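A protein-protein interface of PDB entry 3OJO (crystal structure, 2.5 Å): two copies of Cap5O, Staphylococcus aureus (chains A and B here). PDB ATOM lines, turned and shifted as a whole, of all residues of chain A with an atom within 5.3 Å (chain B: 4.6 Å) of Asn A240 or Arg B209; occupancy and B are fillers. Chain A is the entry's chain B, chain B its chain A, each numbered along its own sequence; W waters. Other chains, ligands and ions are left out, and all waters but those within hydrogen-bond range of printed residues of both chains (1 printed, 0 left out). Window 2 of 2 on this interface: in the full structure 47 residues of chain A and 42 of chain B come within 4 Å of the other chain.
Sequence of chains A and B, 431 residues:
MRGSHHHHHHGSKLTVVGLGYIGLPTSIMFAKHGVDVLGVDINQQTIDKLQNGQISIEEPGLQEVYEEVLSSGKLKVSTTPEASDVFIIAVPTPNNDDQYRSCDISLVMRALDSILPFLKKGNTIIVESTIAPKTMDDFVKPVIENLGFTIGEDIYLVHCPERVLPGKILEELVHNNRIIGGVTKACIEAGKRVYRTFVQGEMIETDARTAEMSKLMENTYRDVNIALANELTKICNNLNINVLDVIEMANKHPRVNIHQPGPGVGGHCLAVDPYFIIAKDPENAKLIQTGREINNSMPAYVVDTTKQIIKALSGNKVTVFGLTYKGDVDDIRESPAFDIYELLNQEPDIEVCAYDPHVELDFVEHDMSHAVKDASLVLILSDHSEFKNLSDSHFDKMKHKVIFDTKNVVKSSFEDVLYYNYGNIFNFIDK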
ATOM      1  N   CYS A 236     -18.931  16.929  29.039  1.00  0.00           N
ATOM      2  CA  CYS A 236     -19.223  16.538  27.661  1.00  0.00           C
ATOM      3  C   CYS A 236     -18.228  15.554  27.116  1.00  0.00           C
ATOM      4  O   CYS A 236     -18.617  14.647  26.381  1.00  0.00           O
ATOM      5  CB  CYS A 236     -19.321  17.760  26.760  1.00  0.00           C
ATOM      6  SG  CYS A 236     -20.889  18.626  26.878  1.00  0.00           S
ATOM      7  N   ASN A 237     -16.949  15.735  27.443  1.00  0.00           N
ATOM      8  CA  ASN A 237     -15.937  14.795  26.969  1.00  0.00           C
ATOM      9  C   ASN A 237     -16.089  13.412  27.610  1.00  0.00           C
ATOM     10  O   ASN A 237     -15.945  12.407  26.912  1.00  0.00           O
ATOM     11  CB  ASN A 237     -14.529  15.355  27.069  1.00  0.00           C
ATOM     12  CG  ASN A 237     -14.148  16.183  25.854  1.00  0.00           C
ATOM     13  OD1 ASN A 237     -13.973  17.399  25.929  1.00  0.00           O
ATOM     14  ND2 ASN A 237     -14.013  15.543  24.706  1.00  0.00           N
ATOM     15  N   ASN A 238     -16.525  13.377  28.886  1.00  0.00           N
ATOM     16  CA  ASN A 238     -16.784  12.153  29.635  1.00  0.00           C
ATOM     17  C   ASN A 238     -17.989  11.385  29.138  1.00  0.00           C
ATOM     18  O   ASN A 238     -18.049  10.174  29.341  1.00  0.00           O
ATOM     19  CB  ASN A 238     -16.930  12.441  31.136  1.00  0.00           C
ATOM     20  CG  ASN A 238     -15.613  12.500  31.882  1.00  0.00           C
ATOM     21  OD1 ASN A 238     -14.514  12.316  31.324  1.00  0.00           O
ATOM     22  ND2 ASN A 238     -15.693  12.727  33.178  1.00  0.00           N
ATOM     23  N   LEU A 239     -18.956  12.074  28.519  1.00  0.00           N
ATOM     24  CA  LEU A 239     -20.198  11.474  28.029  1.00  0.00           C
ATOM     25  C   LEU A 239     -20.246  11.354  26.500  1.00  0.00           C
ATOM     26  O   LEU A 239     -21.296  11.021  25.952  1.00  0.00           O
ATOM     27  CB  LEU A 239     -21.417  12.275  28.524  1.00  0.00           C
ATOM     28  CG  LEU A 239     -21.555  12.565  30.021  1.00  0.00           C
ATOM     29  CD1 LEU A 239     -22.680  13.543  30.259  1.00  0.00           C
ATOM     30  CD2 LEU A 239     -21.816  11.296  30.807  1.00  0.00           C
ATOM     31  N   ASN A 240     -19.123  11.617  25.810  1.00  0.00           N
ATOM     32  CA  ASN A 240     -19.043  11.570  24.348  1.00  0.00           C
ATOM     33  C   ASN A 240     -20.064  12.478  23.708  1.00  0.00           C
ATOM     34  O   ASN A 240     -20.771  12.089  22.778  1.00  0.00           O
ATOM     35  CB  ASN A 240     -19.112  10.131  23.799  1.00  0.00           C
ATOM     36  CG  ASN A 240     -17.923   9.258  24.155  1.00  0.00           C
ATOM     37  OD1 ASN A 240     -17.010   9.647  24.911  1.00  0.00           O
ATOM     38  ND2 ASN A 240     -17.929   8.042  23.629  1.00  0.00           N
ATOM     39  N   ILE A 241     -20.159  13.696  24.250  1.00  0.00           N
ATOM     40  CA  ILE A 241     -21.030  14.754  23.789  1.00  0.00           C
ATOM     41  C   ILE A 241     -20.102  15.858  23.238  1.00  0.00           C
ATOM     42  O   ILE A 241     -18.996  16.074  23.766  1.00  0.00           O
ATOM     43  CB  ILE A 241     -21.999  15.236  24.907  1.00  0.00           C
ATOM     44  CG1 ILE A 241     -22.996  14.106  25.284  1.00  0.00           C
ATOM     45  CG2 ILE A 241     -22.768  16.502  24.486  1.00  0.00           C
ATOM     46  CD1 ILE A 241     -23.799  14.346  26.604  1.00  0.00           C
ATOM     47  N   ASN A 242     -20.520  16.492  22.126  1.00  0.00           N
ATOM     48  CA  ASN A 242     -19.762  17.576  21.535  1.00  0.00           C
ATOM     49  C   ASN A 242     -20.134  18.861  22.289  1.00  0.00           C
ATOM     50  O   ASN A 242     -21.278  19.309  22.200  1.00  0.00           O
ATOM     51  CB  ASN A 242     -20.065  17.696  20.024  1.00  0.00           C
ATOM     52  CG  ASN A 242     -19.170  18.699  19.351  1.00  0.00           C
ATOM     53  OD1 ASN A 242     -19.047  19.867  19.755  1.00  0.00           O
ATOM     54  ND2 ASN A 242     -18.474  18.251  18.350  1.00  0.00           N
ATOM     55  N   VAL A 246     -23.329  21.742  21.430  1.00  0.00           N
ATOM     56  CA  VAL A 246     -24.301  21.962  22.494  1.00  0.00           C
ATOM     57  C   VAL A 246     -24.332  23.440  22.940  1.00  0.00           C
ATOM     58  O   VAL A 246     -25.423  23.989  23.155  1.00  0.00           O
ATOM     59  CB  VAL A 246     -24.115  20.948  23.640  1.00  0.00           C
ATOM     60  CG1 VAL A 246     -25.170  21.148  24.716  1.00  0.00           C
ATOM     61  CG2 VAL A 246     -24.205  19.522  23.098  1.00  0.00           C
ATOM     62  N   PHE A 426     -12.693  13.296  22.375  1.00  0.00           N
ATOM     63  CA  PHE A 426     -13.072  11.983  22.929  1.00  0.00           C
ATOM     64  C   PHE A 426     -13.075  10.844  21.867  1.00  0.00           C
ATOM     65  O   PHE A 426     -12.990   9.675  22.241  1.00  0.00           O
ATOM     66  CB  PHE A 426     -14.438  12.062  23.647  1.00  0.00           C
ATOM     67  CG  PHE A 426     -15.570  12.548  22.772  1.00  0.00           C
ATOM     68  CD1 PHE A 426     -16.267  11.667  21.950  1.00  0.00           C
ATOM     69  CD2 PHE A 426     -15.936  13.889  22.763  1.00  0.00           C
ATOM     70  CE1 PHE A 426     -17.296  12.122  21.129  1.00  0.00           C
ATOM     71  CE2 PHE A 426     -16.975  14.335  21.957  1.00  0.00           C
ATOM     72  CZ  PHE A 426     -17.641  13.454  21.136  1.00  0.00           C
ATOM     73  N   LYS B 134     -27.463  11.448  28.279  1.00  0.00           N
ATOM     74  CA  LYS B 134     -27.216  10.019  28.033  1.00  0.00           C
ATOM     75  C   LYS B 134     -28.269   9.034  28.558  1.00  0.00           C
ATOM     76  O   LYS B 134     -28.063   7.835  28.460  1.00  0.00           O
ATOM     77  CB  LYS B 134     -25.755   9.595  28.268  1.00  0.00           C
ATOM     78  CG  LYS B 134     -24.749  10.353  27.346  1.00  0.00           C
ATOM     79  CD  LYS B 134     -24.469   9.776  25.915  1.00  0.00           C
ATOM     80  CE  LYS B 134     -23.777   8.445  25.863  1.00  0.00           C
ATOM     81  NZ  LYS B 134     -22.318   8.535  25.754  1.00  0.00           N
ATOM     82  N   ASP B 137     -29.877   7.243  25.289  1.00  0.00           N
ATOM     83  CA  ASP B 137     -28.861   6.336  24.755  1.00  0.00           C
ATOM     84  C   ASP B 137     -28.432   5.219  25.682  1.00  0.00           C
ATOM     85  O   ASP B 137     -28.311   4.089  25.212  1.00  0.00           O
ATOM     86  CB  ASP B 137     -27.633   7.128  24.257  1.00  0.00           C
ATOM     87  CG  ASP B 137     -27.911   7.953  23.015  1.00  0.00           C
ATOM     88  OD1 ASP B 137     -28.124   9.175  23.153  1.00  0.00           O
ATOM     89  OD2 ASP B 137     -27.935   7.366  21.899  1.00  0.00           O
ATOM     90  N   ASP B 207     -29.698  15.281  17.870  1.00  0.00           N
ATOM     91  CA  ASP B 207     -29.712  13.966  18.496  1.00  0.00           C
ATOM     92  C   ASP B 207     -30.078  14.105  19.997  1.00  0.00           C
ATOM     93  O   ASP B 207     -29.948  15.197  20.576  1.00  0.00           O
ATOM     94  CB  ASP B 207     -28.408  13.180  18.250  1.00  0.00           C
ATOM     95  CG  ASP B 207     -27.162  13.748  18.904  1.00  0.00           C
ATOM     96  OD1 ASP B 207     -27.238  14.860  19.447  1.00  0.00           O
ATOM     97  OD2 ASP B 207     -26.126  13.046  18.927  1.00  0.00           O
ATOM     98  N   ALA B 208     -30.584  13.013  20.595  1.00  0.00           N
ATOM     99  CA  ALA B 208     -31.058  12.950  21.971  1.00  0.00           C
ATOM    100  C   ALA B 208     -30.066  13.483  22.993  1.00  0.00           C
ATOM    101  O   ALA B 208     -30.469  14.272  23.837  1.00  0.00           O
ATOM    102  CB  ALA B 208     -31.506  11.541  22.310  1.00  0.00           C
ATOM    103  N   ARG B 209     -28.778  13.130  22.890  1.00  0.00           N
ATOM    104  CA  ARG B 209     -27.748  13.602  23.825  1.00  0.00           C
ATOM    105  C   ARG B 209     -27.551  15.136  23.786  1.00  0.00           C
ATOM    106  O   ARG B 209     -27.313  15.734  24.825  1.00  0.00           O
ATOM    107  CB  ARG B 209     -26.414  12.839  23.635  1.00  0.00           C
ATOM    108  CG  ARG B 209     -25.651  13.130  22.321  1.00  0.00           C
ATOM    109  CD  ARG B 209     -24.438  12.244  22.167  1.00  0.00           C
ATOM    110  NE  ARG B 209     -24.822  10.875  21.832  1.00  0.00           N
ATOM    111  CZ  ARG B 209     -24.047   9.816  22.021  1.00  0.00           C
ATOM    112  NH1 ARG B 209     -22.823   9.960  22.526  1.00  0.00           N
ATOM    113  NH2 ARG B 209     -24.487   8.601  21.712  1.00  0.00           N
ATOM    114  N   THR B 210     -27.667  15.760  22.589  1.00  0.00           N
ATOM    115  CA  THR B 210     -27.551  17.204  22.401  1.00  0.00           C
ATOM    116  C   THR B 210     -28.762  17.899  23.005  1.00  0.00           C
ATOM    117  O   THR B 210     -28.577  18.936  23.612  1.00  0.00           O
ATOM    118  CB  THR B 210     -27.284  17.563  20.931  1.00  0.00           C
ATOM    119  OG1 THR B 210     -26.071  16.934  20.518  1.00  0.00           O
ATOM    120  CG2 THR B 210     -27.163  19.061  20.685  1.00  0.00           C
ATOM    121  N   ALA B 211     -29.973  17.326  22.864  1.00  0.00           N
ATOM    122  CA  ALA B 211     -31.218  17.844  23.442  1.00  0.00           C
ATOM    123  C   ALA B 211     -31.162  17.800  24.996  1.00  0.00           C
ATOM    124  O   ALA B 211     -31.657  18.711  25.659  1.00  0.00           O
ATOM    125  CB  ALA B 211     -32.400  17.024  22.948  1.00  0.00           C
ATOM    126  N   GLU B 212     -30.561  16.743  25.571  1.00  0.00           N
ATOM    127  CA  GLU B 212     -30.466  16.588  27.027  1.00  0.00           C
ATOM    128  C   GLU B 212     -29.463  17.591  27.604  1.00  0.00           C
ATOM    129  O   GLU B 212     -29.777  18.288  28.572  1.00  0.00           O
ATOM    130  CB  GLU B 212     -30.046  15.158  27.393  1.00  0.00           C
ATOM    131  CG  GLU B 212     -31.086  14.098  27.087  1.00  0.00           C
ATOM    132  CD  GLU B 212     -30.592  12.661  27.064  1.00  0.00           C
ATOM    133  OE1 GLU B 212     -31.424  11.763  27.298  1.00  0.00           O
ATOM    134  OE2 GLU B 212     -29.395  12.418  26.787  1.00  0.00           O
ATOM    135  N   MET B 213     -28.269  17.655  26.994  1.00  0.00           N
ATOM    136  CA  MET B 213     -27.161  18.514  27.390  1.00  0.00           C
ATOM    137  C   MET B 213     -27.493  20.003  27.276  1.00  0.00           C
ATOM    138  O   MET B 213     -27.216  20.774  28.200  1.00  0.00           O
ATOM    139  CB  MET B 213     -25.896  18.139  26.602  1.00  0.00           C
ATOM    140  CG  MET B 213     -24.616  18.613  27.229  1.00  0.00           C
ATOM    141  SD  MET B 213     -24.579  18.425  29.001  1.00  0.00           S
ATOM    142  CE  MET B 213     -23.145  19.160  29.334  1.00  0.00           C
HETATM  143  O   HOH W   1     -23.093  15.893  20.746  1.00  0.00           O
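The guanidinium group (NH1) of Arg B209 is in hydrogen-bond range of the backbone carbonyl oxygen (O) of Asn A240, 3.0 Å away.
O of Leu A239 sits at hydrogen-bond distance from NZ of Lys B134 (2.7 Å).
Among the printed residues, merely in contact across the chains: Cys A236 with Met B213 (3.4 Å), Leu A239 with Arg B209 (3.9 Å), Ile A241 with Arg B209 (3.9 Å), Ile A241 with Met B213 (3.9 Å), Val A246 with Thr B210 (3.8 Å) and Val A246 with Met B213 (3.6 Å).
Asn A238 touches none of the printed residues of chain B.
Printed residues of chain A within 4 Å of Lys B134: Leu A239 (2.7 Å).
Ala B208 touches none of the printed residues of chain A.
Printed residues of chain A within 4 Å of Arg B209: Leu A239, Asn A240 and Ile A241.
Of the printed residues of chain A, Met B213 touches Cys A236 (3.4 Å), Ile A241 (3.9 Å) and Val A246 (3.6 Å).
The nearest residue of chain A that does not touch Arg B209 is Val A246 (5.2 Å).
Water W1 bridges N of Asn A242 and OG1 of Thr B210.
The side-chain hydroxyl (OG1) of Thr B210 sits at hydrogen-bond distance from the side-chain carboxylate (OD1) of Asp B207 (2.6 Å).
The side-chain carboxylate (OD2) of Asp B207 lies within salt-bridge range of the guanidinium group (NE) of Arg B209 (3.9 Å).
The side-chain carboxylate (OD2) of Asp B137 is in salt-bridge range of the guanidinium group (NH2) of Arg B209, at 3.7 Å.
N of Lys B134 is in hydrogen-bond range of OE2 of Glu B212 (2.6 Å).
The backbone carbonyl oxygen of Cys A236 is in hydrogen-bond range of the backbone NH of Ile A241, at 2.8 Å.
No position is printed for both chains.
Hydrophobic or aromatic side chains of chain A that line the printed part of chain B: Ile A241 and Val A246.
Among the printed residues, 8 pairs touch across the chains.
Among the printed residues, no Asp or Glu carboxylate lies within 4 Å of a Lys or Arg side-chain nitrogen of the other chain.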
